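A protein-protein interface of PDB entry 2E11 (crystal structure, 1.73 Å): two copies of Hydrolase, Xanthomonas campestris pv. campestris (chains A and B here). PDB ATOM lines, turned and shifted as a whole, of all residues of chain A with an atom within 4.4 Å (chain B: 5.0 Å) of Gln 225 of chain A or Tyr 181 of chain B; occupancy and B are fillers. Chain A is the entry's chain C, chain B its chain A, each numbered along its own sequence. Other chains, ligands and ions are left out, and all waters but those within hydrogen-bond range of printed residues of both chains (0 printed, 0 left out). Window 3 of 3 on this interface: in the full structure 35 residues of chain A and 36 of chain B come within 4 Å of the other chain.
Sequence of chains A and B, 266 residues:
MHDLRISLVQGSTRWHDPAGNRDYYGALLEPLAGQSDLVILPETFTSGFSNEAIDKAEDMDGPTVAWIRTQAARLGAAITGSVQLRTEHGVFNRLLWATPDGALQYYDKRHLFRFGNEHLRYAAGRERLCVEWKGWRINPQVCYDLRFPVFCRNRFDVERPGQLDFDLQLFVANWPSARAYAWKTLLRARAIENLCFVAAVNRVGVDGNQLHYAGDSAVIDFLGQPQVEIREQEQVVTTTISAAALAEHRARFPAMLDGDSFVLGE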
ATOM      1  N   ARG A 188     -13.925  19.298 -12.575  1.00  0.00           N
ATOM      2  CA  ARG A 188     -13.038  18.202 -12.957  1.00  0.00           C
ATOM      3  C   ARG A 188     -13.089  17.922 -14.458  1.00  0.00           C
ATOM      4  O   ARG A 188     -12.039  17.730 -15.108  1.00  0.00           O
ATOM      5  CB  ARG A 188     -13.360  16.956 -12.121  1.00  0.00           C
ATOM      6  CG  ARG A 188     -12.928  17.125 -10.638  1.00  0.00           C
ATOM      7  CD  ARG A 188     -13.811  16.337  -9.693  1.00  0.00           C
ATOM      8  NE  ARG A 188     -13.334  16.485  -8.315  1.00  0.00           N
ATOM      9  CZ  ARG A 188     -13.521  17.563  -7.550  1.00  0.00           C
ATOM     10  NH1 ARG A 188     -14.183  18.636  -8.003  1.00  0.00           N
ATOM     11  NH2 ARG A 188     -13.020  17.569  -6.306  1.00  0.00           N
ATOM     12  N   ILE A 192     -10.039  18.269 -17.411  1.00  0.00           N
ATOM     13  CA  ILE A 192      -9.704  17.115 -18.254  1.00  0.00           C
ATOM     14  C   ILE A 192      -9.809  17.468 -19.729  1.00  0.00           C
ATOM     15  O   ILE A 192      -8.852  17.251 -20.503  1.00  0.00           O
ATOM     16  CB  ILE A 192     -10.641  15.910 -17.971  1.00  0.00           C
ATOM     17  CG1 ILE A 192     -10.370  15.353 -16.565  1.00  0.00           C
ATOM     18  CG2 ILE A 192     -10.436  14.834 -19.058  1.00  0.00           C
ATOM     19  CD1 ILE A 192     -11.473  14.351 -16.079  1.00  0.00           C
ATOM     20  N   ILE A 220      -7.421  22.030  -9.254  1.00  0.00           N
ATOM     21  CA  ILE A 220      -7.575  20.730  -9.884  1.00  0.00           C
ATOM     22  C   ILE A 220      -6.551  20.670 -11.013  1.00  0.00           C
ATOM     23  O   ILE A 220      -6.382  21.639 -11.750  1.00  0.00           O
ATOM     24  CB  ILE A 220      -8.996  20.583 -10.442  1.00  0.00           C
ATOM     25  CG1 ILE A 220     -10.010  20.511  -9.277  1.00  0.00           C
ATOM     26  CG2 ILE A 220      -9.106  19.336 -11.318  1.00  0.00           C
ATOM     27  CD1 ILE A 220     -11.343  21.056  -9.621  1.00  0.00           C
ATOM     28  N   ASP A 221      -5.845  19.551 -11.125  1.00  0.00           N
ATOM     29  CA  ASP A 221      -4.799  19.422 -12.133  1.00  0.00           C
ATOM     30  C   ASP A 221      -5.413  19.055 -13.496  1.00  0.00           C
ATOM     31  O   ASP A 221      -6.621  18.820 -13.612  1.00  0.00           O
ATOM     32  CB  ASP A 221      -3.664  18.455 -11.678  1.00  0.00           C
ATOM     33  CG  ASP A 221      -4.088  16.974 -11.694  1.00  0.00           C
ATOM     34  OD1 ASP A 221      -5.084  16.610 -12.370  1.00  0.00           O
ATOM     35  OD2 ASP A 221      -3.382  16.147 -11.072  1.00  0.00           O
ATOM     36  N   LEU A 223      -5.377  16.450 -15.151  1.00  0.00           N
ATOM     37  CA  LEU A 223      -6.007  15.137 -15.212  1.00  0.00           C
ATOM     38  C   LEU A 223      -7.383  15.096 -14.509  1.00  0.00           C
ATOM     39  O   LEU A 223      -8.025  14.025 -14.416  1.00  0.00           O
ATOM     40  CB  LEU A 223      -5.079  14.069 -14.611  1.00  0.00           C
ATOM     41  CG  LEU A 223      -3.809  13.781 -15.433  1.00  0.00           C
ATOM     42  CD1 LEU A 223      -2.863  12.890 -14.675  1.00  0.00           C
ATOM     43  CD2 LEU A 223      -4.148  13.153 -16.760  1.00  0.00           C
ATOM     44  N   GLY A 224      -7.823  16.253 -14.023  1.00  0.00           N
ATOM     45  CA  GLY A 224      -9.092  16.340 -13.309  1.00  0.00           C
ATOM     46  C   GLY A 224      -9.003  15.946 -11.844  1.00  0.00           C
ATOM     47  O   GLY A 224     -10.025  15.834 -11.168  1.00  0.00           O
ATOM     48  N   GLN A 225      -7.780  15.800 -11.347  1.00  0.00           N
ATOM     49  CA  GLN A 225      -7.543  15.358  -9.970  1.00  0.00           C
ATOM     50  C   GLN A 225      -7.267  16.568  -9.089  1.00  0.00           C
ATOM     51  O   GLN A 225      -6.360  17.360  -9.392  1.00  0.00           O
ATOM     52  CB  GLN A 225      -6.349  14.388  -9.910  1.00  0.00           C
ATOM     53  CG  GLN A 225      -6.601  13.039 -10.594  1.00  0.00           C
ATOM     54  CD  GLN A 225      -7.591  12.169  -9.829  1.00  0.00           C
ATOM     55  OE1 GLN A 225      -7.915  12.440  -8.673  1.00  0.00           O
ATOM     56  NE2 GLN A 225      -8.087  11.118 -10.489  1.00  0.00           N
ATOM     57  N   PRO A 226      -8.014  16.710  -7.988  1.00  0.00           N
ATOM     58  CA  PRO A 226      -7.742  17.852  -7.138  1.00  0.00           C
ATOM     59  C   PRO A 226      -6.340  17.754  -6.525  1.00  0.00           C
ATOM     60  O   PRO A 226      -5.807  16.651  -6.272  1.00  0.00           O
ATOM     61  CB  PRO A 226      -8.846  17.781  -6.070  1.00  0.00           C
ATOM     62  CG  PRO A 226      -9.222  16.388  -6.040  1.00  0.00           C
ATOM     63  CD  PRO A 226      -9.123  15.898  -7.453  1.00  0.00           C
ATOM     64  N   GLN A 227      -5.731  18.909  -6.338  1.00  0.00           N
ATOM     65  CA  GLN A 227      -4.481  18.997  -5.629  1.00  0.00           C
ATOM     66  C   GLN A 227      -4.769  19.518  -4.216  1.00  0.00           C
ATOM     67  O   GLN A 227      -4.182  19.044  -3.239  1.00  0.00           O
ATOM     68  CB  GLN A 227      -3.557  19.934  -6.406  1.00  0.00           C
ATOM     69  CG  GLN A 227      -2.217  20.170  -5.794  1.00  0.00           C
ATOM     70  CD  GLN A 227      -1.337  20.948  -6.751  1.00  0.00           C
ATOM     71  OE1 GLN A 227      -1.157  20.542  -7.897  1.00  0.00           O
ATOM     72  NE2 GLN A 227      -0.815  22.079  -6.297  1.00  0.00           N
ATOM     73  N   ARG B 179      -7.065   5.174 -17.386  1.00  0.00           N
ATOM     74  CA  ARG B 179      -7.707   6.489 -17.572  1.00  0.00           C
ATOM     75  C   ARG B 179      -9.202   6.416 -17.274  1.00  0.00           C
ATOM     76  O   ARG B 179      -9.994   7.241 -17.747  1.00  0.00           O
ATOM     77  CB  ARG B 179      -7.413   7.019 -18.983  1.00  0.00           C
ATOM     78  CG  ARG B 179      -5.883   7.206 -19.203  1.00  0.00           C
ATOM     79  CD  ARG B 179      -5.495   7.893 -20.505  1.00  0.00           C
ATOM     80  NE  ARG B 179      -5.906   7.121 -21.680  1.00  0.00           N
ATOM     81  CZ  ARG B 179      -5.242   6.089 -22.203  1.00  0.00           C
ATOM     82  NH1 ARG B 179      -5.742   5.490 -23.269  1.00  0.00           N
ATOM     83  NH2 ARG B 179      -4.102   5.645 -21.658  1.00  0.00           N
ATOM     84  N   ALA B 180      -9.593   5.445 -16.450  1.00  0.00           N
ATOM     85  CA  ALA B 180     -11.017   5.282 -16.113  1.00  0.00           C
ATOM     86  C   ALA B 180     -11.584   6.521 -15.453  1.00  0.00           C
ATOM     87  O   ALA B 180     -12.749   6.845 -15.640  1.00  0.00           O
ATOM     88  CB  ALA B 180     -11.227   4.095 -15.215  1.00  0.00           C
ATOM     89  N   TYR B 181     -10.770   7.205 -14.659  1.00  0.00           N
ATOM     90  CA  TYR B 181     -11.277   8.401 -13.986  1.00  0.00           C
ATOM     91  C   TYR B 181     -11.815   9.414 -14.991  1.00  0.00           C
ATOM     92  O   TYR B 181     -12.874   9.997 -14.761  1.00  0.00           O
ATOM     93  CB  TYR B 181     -10.179   9.038 -13.144  1.00  0.00           C
ATOM     94  CG  TYR B 181     -10.586  10.332 -12.495  1.00  0.00           C
ATOM     95  CD1 TYR B 181     -11.357  10.326 -11.341  1.00  0.00           C
ATOM     96  CD2 TYR B 181     -10.184  11.566 -13.019  1.00  0.00           C
ATOM     97  CE1 TYR B 181     -11.722  11.506 -10.724  1.00  0.00           C
ATOM     98  CE2 TYR B 181     -10.560  12.768 -12.411  1.00  0.00           C
ATOM     99  CZ  TYR B 181     -11.320  12.722 -11.265  1.00  0.00           C
ATOM    100  OH  TYR B 181     -11.659  13.894 -10.613  1.00  0.00           O
ATOM    101  N   ALA B 182     -11.091   9.618 -16.102  1.00  0.00           N
ATOM    102  CA  ALA B 182     -11.526  10.565 -17.118  1.00  0.00           C
ATOM    103  C   ALA B 182     -12.845  10.115 -17.777  1.00  0.00           C
ATOM    104  O   ALA B 182     -13.729  10.925 -18.012  1.00  0.00           O
ATOM    105  CB  ALA B 182     -10.431  10.795 -18.156  1.00  0.00           C
ATOM    106  N   TRP B 183     -12.950   8.830 -18.069  1.00  0.00           N
ATOM    107  CA  TRP B 183     -14.177   8.233 -18.604  1.00  0.00           C
ATOM    108  C   TRP B 183     -15.365   8.537 -17.704  1.00  0.00           C
ATOM    109  O   TRP B 183     -16.350   9.129 -18.146  1.00  0.00           O
ATOM    110  CB  TRP B 183     -13.980   6.721 -18.706  1.00  0.00           C
ATOM    111  CG  TRP B 183     -15.175   5.870 -18.991  1.00  0.00           C
ATOM    112  CD1 TRP B 183     -15.838   5.076 -18.089  1.00  0.00           C
ATOM    113  CD2 TRP B 183     -15.849   5.685 -20.258  1.00  0.00           C
ATOM    114  NE1 TRP B 183     -16.880   4.421 -18.718  1.00  0.00           N
ATOM    115  CE2 TRP B 183     -16.891   4.753 -20.043  1.00  0.00           C
ATOM    116  CE3 TRP B 183     -15.668   6.210 -21.544  1.00  0.00           C
ATOM    117  CZ2 TRP B 183     -17.770   4.357 -21.060  1.00  0.00           C
ATOM    118  CZ3 TRP B 183     -16.539   5.803 -22.567  1.00  0.00           C
ATOM    119  CH2 TRP B 183     -17.569   4.885 -22.311  1.00  0.00           C
ATOM    120  N   LYS B 184     -15.259   8.146 -16.437  1.00  0.00           N
ATOM    121  CA  LYS B 184     -16.372   8.314 -15.491  1.00  0.00           C
ATOM    122  C   LYS B 184     -16.760   9.775 -15.341  1.00  0.00           C
ATOM    123  O   LYS B 184     -17.931  10.131 -15.386  1.00  0.00           O
ATOM    124  CB  LYS B 184     -16.016   7.707 -14.139  1.00  0.00           C
ATOM    125  CG  LYS B 184     -15.740   6.179 -14.216  1.00  0.00           C
ATOM    126  CD  LYS B 184     -15.167   5.647 -12.904  1.00  0.00           C
ATOM    127  CE  LYS B 184     -16.212   5.640 -11.803  1.00  0.00           C
ATOM    128  NZ  LYS B 184     -17.062   4.403 -11.837  1.00  0.00           N
ATOM    129  N   THR B 185     -15.756  10.632 -15.239  1.00  0.00           N
ATOM    130  CA  THR B 185     -15.997  12.039 -14.990  1.00  0.00           C
ATOM    131  C   THR B 185     -16.663  12.707 -16.197  1.00  0.00           C
ATOM    132  O   THR B 185     -17.651  13.423 -16.051  1.00  0.00           O
ATOM    133  CB  THR B 185     -14.675  12.752 -14.628  1.00  0.00           C
ATOM    134  OG1 THR B 185     -14.194  12.236 -13.373  1.00  0.00           O
ATOM    135  CG2 THR B 185     -14.904  14.275 -14.465  1.00  0.00           C
ATOM    136  N   LEU B 186     -16.119  12.462 -17.381  1.00  0.00           N
ATOM    137  CA  LEU B 186     -16.659  13.098 -18.580  1.00  0.00           C
ATOM    138  C   LEU B 186     -18.089  12.678 -18.900  1.00  0.00           C
ATOM    139  O   LEU B 186     -18.890  13.506 -19.295  1.00  0.00           O
ATOM    140  CB  LEU B 186     -15.729  12.887 -19.766  1.00  0.00           C
ATOM    141  CG  LEU B 186     -14.389  13.625 -19.661  1.00  0.00           C
ATOM    142  CD1 LEU B 186     -13.468  13.248 -20.818  1.00  0.00           C
ATOM    143  CD2 LEU B 186     -14.543  15.134 -19.568  1.00  0.00           C
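Arg 188 of chain A touches Tyr 181 of chain B. Thr 185 of chain B touches Arg 188 of chain A (CG2 to CB, 3.9 Å). Ile 192 of chain A touches Ala 182 of chain B (CD1 to CA, 3.9 Å). Thr 185 of chain B touches Ile 192 of chain A. Ile 192 of chain A touches Leu 186 of chain B. O of Leu 223 of chain A touches CE2 of Tyr 181 of chain B (3.5 Å). Gln 225 of chain A touches Tyr 181 of chain B (NE2 to CG, 3.3 Å).
Printed residues of chain B within 4 Å of Arg 188 of chain A: Tyr 181 and Thr 185. Ile 220 of chain A touches none of the printed residues of chain B. Of the printed residues of chain B, Leu 223 of chain A touches Tyr 181 (3.5 Å). Printed residues of chain B within 4 Å of Gln 225 of chain A: Tyr 181. Pro 226 of chain A touches none of the printed residues of chain B. Of the printed residues of chain A, Tyr 181 of chain B touches Arg 188 (3.4 Å), Leu 223 (3.5 Å), Gly 224 (2.6 Å) and Gln 225 (3.3 Å). Printed residues of chain A within 4 Å of Ala 182 of chain B: Ile 192. Printed residues of chain A within 4 Å of Thr 185 of chain B: Arg 188 and Ile 192. Printed residues of chain A within 4 Å of Leu 186 of chain B: Ile 192 (3.8 Å). The nearest residue of chain A that does not touch Tyr 181 of chain B is Ile 192 of chain A (4.1 Å).
No position is printed for both chains.
Printed residues of chain A that touch a printed residue of chain B: Arg 188, Ile 192, Leu 223, Gly 224 and Gln 225. Hydrophobic or aromatic side chains of chain A that line the printed part of chain B: Ile 192. Hydrophobic or aromatic side chains of chain B that line the printed part of chain A: Tyr 181 and Leu 186. Among the printed residues, 8 pairs touch across the chains. Among the printed residues, no Asp or Glu carboxylate lies within 4 Å of a Lys or Arg side-chain nitrogen of the other chain.
The side-chain hydroxyl (OH) of Tyr 181 of chain B sits at hydrogen-bond distance from the backbone carbonyl oxygen (O) of Gly 224 of chain A, at 2.6 Å.
The side-chain hydroxyl of Thr 185 of chain B sits at hydrogen-bond distance from the backbone carbonyl oxygen of Tyr 181 of chain B (2.9 Å). OD1 of Asp 221 of chain A is in hydrogen-bond range of N of Leu 223 of chain A, 2.8 Å away. OD1 of Asp 221 of chain A lies within hydrogen-bond range of N of Gly 224 of chain A, 3.2 Å away. The side-chain carboxylate (OD1) of Asp 221 of chain A sits at hydrogen-bond distance from the backbone NH (N) of Gln 225 of chain A (3.0 Å).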
